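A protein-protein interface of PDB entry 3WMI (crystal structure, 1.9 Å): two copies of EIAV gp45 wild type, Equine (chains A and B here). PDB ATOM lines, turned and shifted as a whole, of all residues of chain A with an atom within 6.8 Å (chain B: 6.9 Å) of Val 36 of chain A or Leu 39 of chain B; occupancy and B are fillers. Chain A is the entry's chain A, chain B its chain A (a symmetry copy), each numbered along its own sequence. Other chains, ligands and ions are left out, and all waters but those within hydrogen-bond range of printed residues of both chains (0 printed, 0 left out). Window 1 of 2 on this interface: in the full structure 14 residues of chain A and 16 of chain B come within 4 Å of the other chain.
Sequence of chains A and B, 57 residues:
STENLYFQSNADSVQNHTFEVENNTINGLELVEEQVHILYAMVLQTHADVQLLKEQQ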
ATOM      1  N   LEU A  31      -9.025  25.066 -30.244  1.00  0.00           N
ATOM      2  CA  LEU A  31     -10.166  24.201 -29.950  1.00  0.00           C
ATOM      3  C   LEU A  31     -10.213  23.837 -28.466  1.00  0.00           C
ATOM      4  O   LEU A  31     -11.276  23.840 -27.871  1.00  0.00           O
ATOM      5  CB  LEU A  31     -10.130  22.932 -30.799  1.00  0.00           C
ATOM      6  CG  LEU A  31     -10.333  23.134 -32.303  1.00  0.00           C
ATOM      7  CD1 LEU A  31      -9.958  21.864 -33.029  1.00  0.00           C
ATOM      8  CD2 LEU A  31     -11.769  23.511 -32.581  1.00  0.00           C
ATOM      9  N   VAL A  32      -9.065  23.498 -27.887  1.00  0.00           N
ATOM     10  CA  VAL A  32      -9.000  23.186 -26.461  1.00  0.00           C
ATOM     11  C   VAL A  32      -9.453  24.398 -25.654  1.00  0.00           C
ATOM     12  O   VAL A  32     -10.215  24.265 -24.690  1.00  0.00           O
ATOM     13  CB  VAL A  32      -7.583  22.747 -26.033  1.00  0.00           C
ATOM     14  CG1 VAL A  32      -7.448  22.738 -24.532  1.00  0.00           C
ATOM     15  CG2 VAL A  32      -7.237  21.372 -26.636  1.00  0.00           C
ATOM     16  N   GLU A  33      -9.017  25.580 -26.070  1.00  0.00           N
ATOM     17  CA  GLU A  33      -9.432  26.820 -25.410  1.00  0.00           C
ATOM     18  C   GLU A  33     -10.945  27.046 -25.476  1.00  0.00           C
ATOM     19  O   GLU A  33     -11.534  27.577 -24.534  1.00  0.00           O
ATOM     20  CB  GLU A  33      -8.682  28.031 -25.978  1.00  0.00           C
ATOM     21  CG  GLU A  33      -9.041  29.375 -25.317  1.00  0.00           C
ATOM     22  CD  GLU A  33      -8.603  29.466 -23.850  1.00  0.00           C
ATOM     23  OE1 GLU A  33      -8.025  28.493 -23.317  1.00  0.00           O
ATOM     24  OE2 GLU A  33      -8.831  30.526 -23.231  1.00  0.00           O
ATOM     25  N   GLU A  34     -11.578  26.639 -26.572  1.00  0.00           N
ATOM     26  CA  GLU A  34     -13.036  26.747 -26.664  1.00  0.00           C
ATOM     27  C   GLU A  34     -13.700  25.799 -25.668  1.00  0.00           C
ATOM     28  O   GLU A  34     -14.720  26.141 -25.062  1.00  0.00           O
ATOM     29  CB  GLU A  34     -13.532  26.469 -28.087  1.00  0.00           C
ATOM     30  CG  GLU A  34     -13.066  27.502 -29.112  1.00  0.00           C
ATOM     31  CD  GLU A  34     -13.604  27.238 -30.507  1.00  0.00           C
ATOM     32  OE1 GLU A  34     -14.627  26.527 -30.630  1.00  0.00           O
ATOM     33  OE2 GLU A  34     -12.999  27.739 -31.488  1.00  0.00           O
ATOM     34  N   GLN A  35     -13.120  24.613 -25.506  1.00  0.00           N
ATOM     35  CA  GLN A  35     -13.582  23.685 -24.479  1.00  0.00           C
ATOM     36  C   GLN A  35     -13.429  24.287 -23.081  1.00  0.00           C
ATOM     37  O   GLN A  35     -14.302  24.115 -22.244  1.00  0.00           O
ATOM     38  CB  GLN A  35     -12.825  22.367 -24.552  1.00  0.00           C
ATOM     39  CG  GLN A  35     -13.099  21.561 -25.800  1.00  0.00           C
ATOM     40  CD  GLN A  35     -12.363  20.261 -25.756  1.00  0.00           C
ATOM     41  OE1 GLN A  35     -11.187  20.242 -25.442  1.00  0.00           O
ATOM     42  NE2 GLN A  35     -13.049  19.165 -26.027  1.00  0.00           N
ATOM     43  N   VAL A  36     -12.317  24.976 -22.833  1.00  0.00           N
ATOM     44  CA  VAL A  36     -12.086  25.617 -21.536  1.00  0.00           C
ATOM     45  C   VAL A  36     -13.200  26.622 -21.246  1.00  0.00           C
ATOM     46  O   VAL A  36     -13.742  26.664 -20.128  1.00  0.00           O
ATOM     47  CB  VAL A  36     -10.691  26.320 -21.475  1.00  0.00           C
ATOM     48  CG1 VAL A  36     -10.618  27.275 -20.286  1.00  0.00           C
ATOM     49  CG2 VAL A  36      -9.552  25.279 -21.411  1.00  0.00           C
ATOM     50  N   HIS A  37     -13.549  27.421 -22.254  1.00  0.00           N
ATOM     51  CA  HIS A  37     -14.620  28.414 -22.116  1.00  0.00           C
ATOM     52  C   HIS A  37     -15.947  27.756 -21.713  1.00  0.00           C
ATOM     53  O   HIS A  37     -16.700  28.292 -20.892  1.00  0.00           O
ATOM     54  CB  HIS A  37     -14.841  29.183 -23.427  1.00  0.00           C
ATOM     55  CG  HIS A  37     -13.676  30.018 -23.864  1.00  0.00           C
ATOM     56  ND1 HIS A  37     -12.683  30.433 -23.007  1.00  0.00           N
ATOM     57  CD2 HIS A  37     -13.354  30.521 -25.083  1.00  0.00           C
ATOM     58  CE1 HIS A  37     -11.800  31.154 -23.672  1.00  0.00           C
ATOM     59  NE2 HIS A  37     -12.178  31.218 -24.938  1.00  0.00           N
ATOM     60  N   ILE A  38     -16.251  26.616 -22.326  1.00  0.00           N
ATOM     61  CA  ILE A  38     -17.485  25.895 -22.029  1.00  0.00           C
ATOM     62  C   ILE A  38     -17.467  25.344 -20.607  1.00  0.00           C
ATOM     63  O   ILE A  38     -18.430  25.502 -19.876  1.00  0.00           O
ATOM     64  CB  ILE A  38     -17.738  24.752 -23.028  1.00  0.00           C
ATOM     65  CG1 ILE A  38     -17.956  25.324 -24.431  1.00  0.00           C
ATOM     66  CG2 ILE A  38     -18.921  23.919 -22.597  1.00  0.00           C
ATOM     67  CD1 ILE A  38     -17.909  24.272 -25.517  1.00  0.00           C
ATOM     68  N   LEU A  39     -16.371  24.702 -20.219  1.00  0.00           N
ATOM     69  CA  LEU A  39     -16.246  24.192 -18.848  1.00  0.00           C
ATOM     70  C   LEU A  39     -16.402  25.327 -17.847  1.00  0.00           C
ATOM     71  O   LEU A  39     -17.060  25.175 -16.809  1.00  0.00           O
ATOM     72  CB  LEU A  39     -14.891  23.518 -18.648  1.00  0.00           C
ATOM     73  CG  LEU A  39     -14.767  22.150 -19.316  1.00  0.00           C
ATOM     74  CD1 LEU A  39     -13.317  21.688 -19.309  1.00  0.00           C
ATOM     75  CD2 LEU A  39     -15.643  21.143 -18.571  1.00  0.00           C
ATOM     76  N   TYR A  40     -15.790  26.464 -18.168  1.00  0.00           N
ATOM     77  CA  TYR A  40     -15.809  27.624 -17.283  1.00  0.00           C
ATOM     78  C   TYR A  40     -17.248  28.092 -17.049  1.00  0.00           C
ATOM     79  O   TYR A  40     -17.656  28.322 -15.908  1.00  0.00           O
ATOM     80  CB  TYR A  40     -14.932  28.733 -17.883  1.00  0.00           C
ATOM     81  CG  TYR A  40     -14.862  30.034 -17.103  1.00  0.00           C
ATOM     82  CD1 TYR A  40     -14.590  30.052 -15.743  1.00  0.00           C
ATOM     83  CD2 TYR A  40     -15.007  31.253 -17.755  1.00  0.00           C
ATOM     84  CE1 TYR A  40     -14.502  31.265 -15.042  1.00  0.00           C
ATOM     85  CE2 TYR A  40     -14.931  32.450 -17.072  1.00  0.00           C
ATOM     86  CZ  TYR A  40     -14.670  32.451 -15.724  1.00  0.00           C
ATOM     87  OH  TYR A  40     -14.594  33.659 -15.074  1.00  0.00           O
ATOM     88  N   ALA A  41     -18.019  28.216 -18.126  1.00  0.00           N
ATOM     89  CA  ALA A  41     -19.429  28.591 -18.011  1.00  0.00           C
ATOM     90  C   ALA A  41     -20.243  27.569 -17.218  1.00  0.00           C
ATOM     91  O   ALA A  41     -21.080  27.952 -16.401  1.00  0.00           O
ATOM     92  CB  ALA A  41     -20.047  28.797 -19.383  1.00  0.00           C
ATOM     93  N   VAL A  43     -19.129  25.601 -14.955  1.00  0.00           N
ATOM     94  CA  VAL A  43     -18.644  25.697 -13.578  1.00  0.00           C
ATOM     95  C   VAL A  43     -19.259  26.904 -12.853  1.00  0.00           C
ATOM     96  O   VAL A  43     -19.688  26.800 -11.695  1.00  0.00           O
ATOM     97  CB  VAL A  43     -17.082  25.732 -13.542  1.00  0.00           C
ATOM     98  CG1 VAL A  43     -16.561  26.298 -12.214  1.00  0.00           C
ATOM     99  CG2 VAL A  43     -16.520  24.328 -13.786  1.00  0.00           C
ATOM    100  N   VAL B  32      -2.931  27.552 -21.150  1.00  0.00           N
ATOM    101  CA  VAL B  32      -4.125  26.712 -21.088  1.00  0.00           C
ATOM    102  C   VAL B  32      -4.051  25.814 -19.858  1.00  0.00           C
ATOM    103  O   VAL B  32      -5.042  25.649 -19.137  1.00  0.00           O
ATOM    104  CB  VAL B  32      -4.300  25.866 -22.367  1.00  0.00           C
ATOM    105  CG1 VAL B  32      -5.332  24.788 -22.168  1.00  0.00           C
ATOM    106  CG2 VAL B  32      -4.654  26.766 -23.567  1.00  0.00           C
ATOM    107  N   GLU B  34      -2.577  26.481 -17.072  1.00  0.00           N
ATOM    108  CA  GLU B  34      -2.865  27.289 -15.884  1.00  0.00           C
ATOM    109  C   GLU B  34      -4.373  27.453 -15.709  1.00  0.00           C
ATOM    110  O   GLU B  34      -4.879  27.434 -14.584  1.00  0.00           O
ATOM    111  CB  GLU B  34      -2.177  28.655 -15.951  1.00  0.00           C
ATOM    112  CG  GLU B  34      -0.651  28.576 -15.927  1.00  0.00           C
ATOM    113  CD  GLU B  34       0.015  29.941 -15.947  1.00  0.00           C
ATOM    114  OE1 GLU B  34      -0.651  30.938 -15.585  1.00  0.00           O
ATOM    115  OE2 GLU B  34       1.207  30.021 -16.333  1.00  0.00           O
ATOM    116  N   GLN B  35      -5.082  27.616 -16.823  1.00  0.00           N
ATOM    117  CA  GLN B  35      -6.540  27.639 -16.790  1.00  0.00           C
ATOM    118  C   GLN B  35      -7.102  26.315 -16.267  1.00  0.00           C
ATOM    119  O   GLN B  35      -8.060  26.316 -15.510  1.00  0.00           O
ATOM    120  CB  GLN B  35      -7.114  27.930 -18.168  1.00  0.00           C
ATOM    121  CG  GLN B  35      -6.825  29.319 -18.682  1.00  0.00           C
ATOM    122  CD  GLN B  35      -7.478  29.533 -20.011  1.00  0.00           C
ATOM    123  OE1 GLN B  35      -7.372  28.688 -20.879  1.00  0.00           O
ATOM    124  NE2 GLN B  35      -8.187  30.636 -20.168  1.00  0.00           N
ATOM    125  N   VAL B  36      -6.513  25.197 -16.687  1.00  0.00           N
ATOM    126  CA  VAL B  36      -6.956  23.879 -16.226  1.00  0.00           C
ATOM    127  C   VAL B  36      -6.839  23.794 -14.704  1.00  0.00           C
ATOM    128  O   VAL B  36      -7.763  23.318 -14.021  1.00  0.00           O
ATOM    129  CB  VAL B  36      -6.144  22.724 -16.896  1.00  0.00           C
ATOM    130  CG1 VAL B  36      -6.354  21.409 -16.150  1.00  0.00           C
ATOM    131  CG2 VAL B  36      -6.527  22.575 -18.385  1.00  0.00           C
ATOM    132  N   HIS B  37      -5.713  24.266 -14.173  1.00  0.00           N
ATOM    133  CA  HIS B  37      -5.483  24.266 -12.723  1.00  0.00           C
ATOM    134  C   HIS B  37      -6.576  25.049 -11.982  1.00  0.00           C
ATOM    135  O   HIS B  37      -7.033  24.642 -10.908  1.00  0.00           O
ATOM    136  CB  HIS B  37      -4.123  24.888 -12.372  1.00  0.00           C
ATOM    137  CG  HIS B  37      -2.939  24.129 -12.890  1.00  0.00           C
ATOM    138  ND1 HIS B  37      -2.993  22.801 -13.250  1.00  0.00           N
ATOM    139  CD2 HIS B  37      -1.658  24.522 -13.102  1.00  0.00           C
ATOM    140  CE1 HIS B  37      -1.803  22.407 -13.659  1.00  0.00           C
ATOM    141  NE2 HIS B  37      -0.972  23.434 -13.588  1.00  0.00           N
ATOM    142  N   ILE B  38      -6.961  26.194 -12.536  1.00  0.00           N
ATOM    143  CA  ILE B  38      -7.992  27.029 -11.927  1.00  0.00           C
ATOM    144  C   ILE B  38      -9.350  26.337 -11.968  1.00  0.00           C
ATOM    145  O   ILE B  38     -10.047  26.293 -10.968  1.00  0.00           O
ATOM    146  CB  ILE B  38      -8.090  28.409 -12.603  1.00  0.00           C
ATOM    147  CG1 ILE B  38      -6.790  29.187 -12.389  1.00  0.00           C
ATOM    148  CG2 ILE B  38      -9.273  29.180 -12.071  1.00  0.00           C
ATOM    149  CD1 ILE B  38      -6.680  30.415 -13.266  1.00  0.00           C
ATOM    150  N   LEU B  39      -9.720  25.794 -13.122  1.00  0.00           N
ATOM    151  CA  LEU B  39     -10.985  25.057 -13.234  1.00  0.00           C
ATOM    152  C   LEU B  39     -11.012  23.904 -12.242  1.00  0.00           C
ATOM    153  O   LEU B  39     -12.036  23.642 -11.598  1.00  0.00           O
ATOM    154  CB  LEU B  39     -11.167  24.515 -14.650  1.00  0.00           C
ATOM    155  CG  LEU B  39     -11.534  25.577 -15.685  1.00  0.00           C
ATOM    156  CD1 LEU B  39     -11.415  25.008 -17.090  1.00  0.00           C
ATOM    157  CD2 LEU B  39     -12.963  26.055 -15.430  1.00  0.00           C
ATOM    158  N   TYR B  40      -9.877  23.220 -12.124  1.00  0.00           N
ATOM    159  CA  TYR B  40      -9.766  22.058 -11.248  1.00  0.00           C
ATOM    160  C   TYR B  40     -10.050  22.456  -9.798  1.00  0.00           C
ATOM    161  O   TYR B  40     -10.829  21.797  -9.106  1.00  0.00           O
ATOM    162  CB  TYR B  40      -8.374  21.430 -11.415  1.00  0.00           C
ATOM    163  CG  TYR B  40      -8.072  20.220 -10.547  1.00  0.00           C
ATOM    164  CD1 TYR B  40      -8.948  19.146 -10.469  1.00  0.00           C
ATOM    165  CD2 TYR B  40      -6.870  20.132  -9.857  1.00  0.00           C
ATOM    166  CE1 TYR B  40      -8.642  18.024  -9.684  1.00  0.00           C
ATOM    167  CE2 TYR B  40      -6.565  19.035  -9.077  1.00  0.00           C
ATOM    168  CZ  TYR B  40      -7.445  17.985  -9.001  1.00  0.00           C
ATOM    169  OH  TYR B  40      -7.109  16.905  -8.221  1.00  0.00           O
ATOM    170  N   ALA B  41      -9.428  23.541  -9.343  1.00  0.00           N
ATOM    171  CA  ALA B  41      -9.678  24.049  -7.994  1.00  0.00           C
ATOM    172  C   ALA B  41     -11.132  24.470  -7.787  1.00  0.00           C
ATOM    173  O   ALA B  41     -11.709  24.187  -6.737  1.00  0.00           O
ATOM    174  CB  ALA B  41      -8.750  25.209  -7.673  1.00  0.00           C
ATOM    175  N   MET B  42     -11.716  25.154  -8.770  1.00  0.00           N
ATOM    176  CA  MET B  42     -13.115  25.563  -8.678  1.00  0.00           C
ATOM    177  C   MET B  42     -13.999  24.337  -8.557  1.00  0.00           C
ATOM    178  O   MET B  42     -14.941  24.319  -7.773  1.00  0.00           O
ATOM    179  CB  MET B  42     -13.540  26.387  -9.901  1.00  0.00           C
ATOM    180  CG  MET B  42     -12.813  27.722 -10.023  1.00  0.00           C
ATOM    181  SD  MET B  42     -13.026  28.502 -11.631  1.00  0.00           S
ATOM    182  CE  MET B  42     -14.312  29.691 -11.279  1.00  0.00           C
ATOM    183  N   VAL B  43     -13.679  23.315  -9.341  1.00  0.00           N
ATOM    184  CA  VAL B  43     -14.455  22.075  -9.380  1.00  0.00           C
ATOM    185  C   VAL B  43     -14.374  21.324  -8.042  1.00  0.00           C
ATOM    186  O   VAL B  43     -15.387  20.831  -7.526  1.00  0.00           O
ATOM    187  CB  VAL B  43     -14.005  21.179 -10.578  1.00  0.00           C
ATOM    188  CG1 VAL B  43     -14.434  19.718 -10.381  1.00  0.00           C
ATOM    189  CG2 VAL B  43     -14.570  21.733 -11.889  1.00  0.00           C
ATOM    190  N   LEU B  44     -13.170  21.254  -7.477  1.00  0.00           N
ATOM    191  CA  LEU B  44     -12.971  20.639  -6.168  1.00  0.00           C
ATOM    192  C   LEU B  44     -13.712  21.398  -5.061  1.00  0.00           C
ATOM    193  O   LEU B  44     -14.315  20.787  -4.168  1.00  0.00           O
ATOM    194  CB  LEU B  44     -11.474  20.555  -5.838  1.00  0.00           C
ATOM    195  CG  LEU B  44     -10.627  19.543  -6.614  1.00  0.00           C
ATOM    196  CD1 LEU B  44      -9.147  19.640  -6.218  1.00  0.00           C
ATOM    197  CD2 LEU B  44     -11.112  18.118  -6.434  1.00  0.00           C
ATOM    198  N   GLN B  45     -13.658  22.723  -5.108  1.00  0.00           N
ATOM    199  CA  GLN B  45     -14.365  23.540  -4.120  1.00  0.00           C
ATOM    200  C   GLN B  45     -15.878  23.346  -4.198  1.00  0.00           C
ATOM    201  O   GLN B  45     -16.545  23.187  -3.177  1.00  0.00           O
ATOM    202  CB  GLN B  45     -14.016  25.019  -4.293  1.00  0.00           C
ATOM    203  CG  GLN B  45     -14.784  25.955  -3.359  1.00  0.00           C
ATOM    204  CD  GLN B  45     -14.383  25.776  -1.915  1.00  0.00           C
ATOM    205  OE1 GLN B  45     -13.223  25.511  -1.620  1.00  0.00           O
ATOM    206  NE2 GLN B  45     -15.348  25.906  -1.003  1.00  0.00           N
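OE1 of Gln 35 of chain B lies close to OE1 of Glu 33 of chain A (2.5 Å).
A ring nitrogen (ND1) of His 37 of chain A lies close to the backbone carbonyl oxygen (O) of Glu 33 of chain A, at 3.4 Å.
Val 32 of chain A touches Val 32 of chain B (CG1 to CG1, 3.8 Å).
OE1 of Glu 33 of chain A touches CG2 of Val 32 of chain B, at 3.8 Å.
Val 36 of chain A touches Gln 35 of chain B.
Val 36 of chain A touches Leu 39 of chain B (CG1 to CD1, 3.999 Å).
Tyr 40 of chain A touches Leu 39 of chain B.
CG1 of Val 43 of chain A touches CB of Met 42 of chain B, 3.8 Å away.
CG2 of Val 43 of chain B touches CG2 of Val 43 of chain A, at 3.8 Å.
Of the printed residues of chain B, Val 36 of chain A touches Gln 35 and Leu 39.
Printed residues of chain B within 4 Å of Val 43 of chain A: Met 42 and Val 43.
Printed residues of chain A within 4 Å of Val 32 of chain B: Val 32 (3.8 Å) and Glu 33 (3.8 Å).
Printed residues of chain A within 4 Å of Val 43 of chain B: Val 43 (3.8 Å).
Ile 38 of chain B touches none of the printed residues of chain A.
Leu 31 of chain A touches none of the printed residues of chain B.
The nearest printed residue of chain A that does not touch Leu 39 of chain B is Leu 39 of chain A (4.1 Å).
Of the 13 printed residues of chain B, 5 touch a printed residue of chain A.
Hydrophobic or aromatic side chains of chain B within 4 Å of the printed part of chain A: Val 32, Leu 39, Met 42 and Val 43.
Hydrophobic or aromatic side chains of chain A within 4 Å of the printed part of chain B: Val 32, Val 36 and Val 43.
Among the printed residues, no Asp or Glu carboxylate lies within 4 Å of a Lys or Arg side-chain nitrogen of the other chain.
Val 32 of chain B touches its own counterpart, Val 32 of chain A.
Val 36 of chain A touches Gln 35 of chain B, but with the chains exchanged Gln 35 of chain A does not touch Val 36 of chain B (8.5 Å).
Val 36 of chain A touches Leu 39 of chain B, but with the chains exchanged Leu 39 of chain A does not touch Val 36 of chain B (6.9 Å).
Tyr 40 of chain A touches Leu 39 of chain B, but with the chains exchanged Leu 39 of chain A does not touch Tyr 40 of chain B (8.1 Å).
10 positions are printed for both chains.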
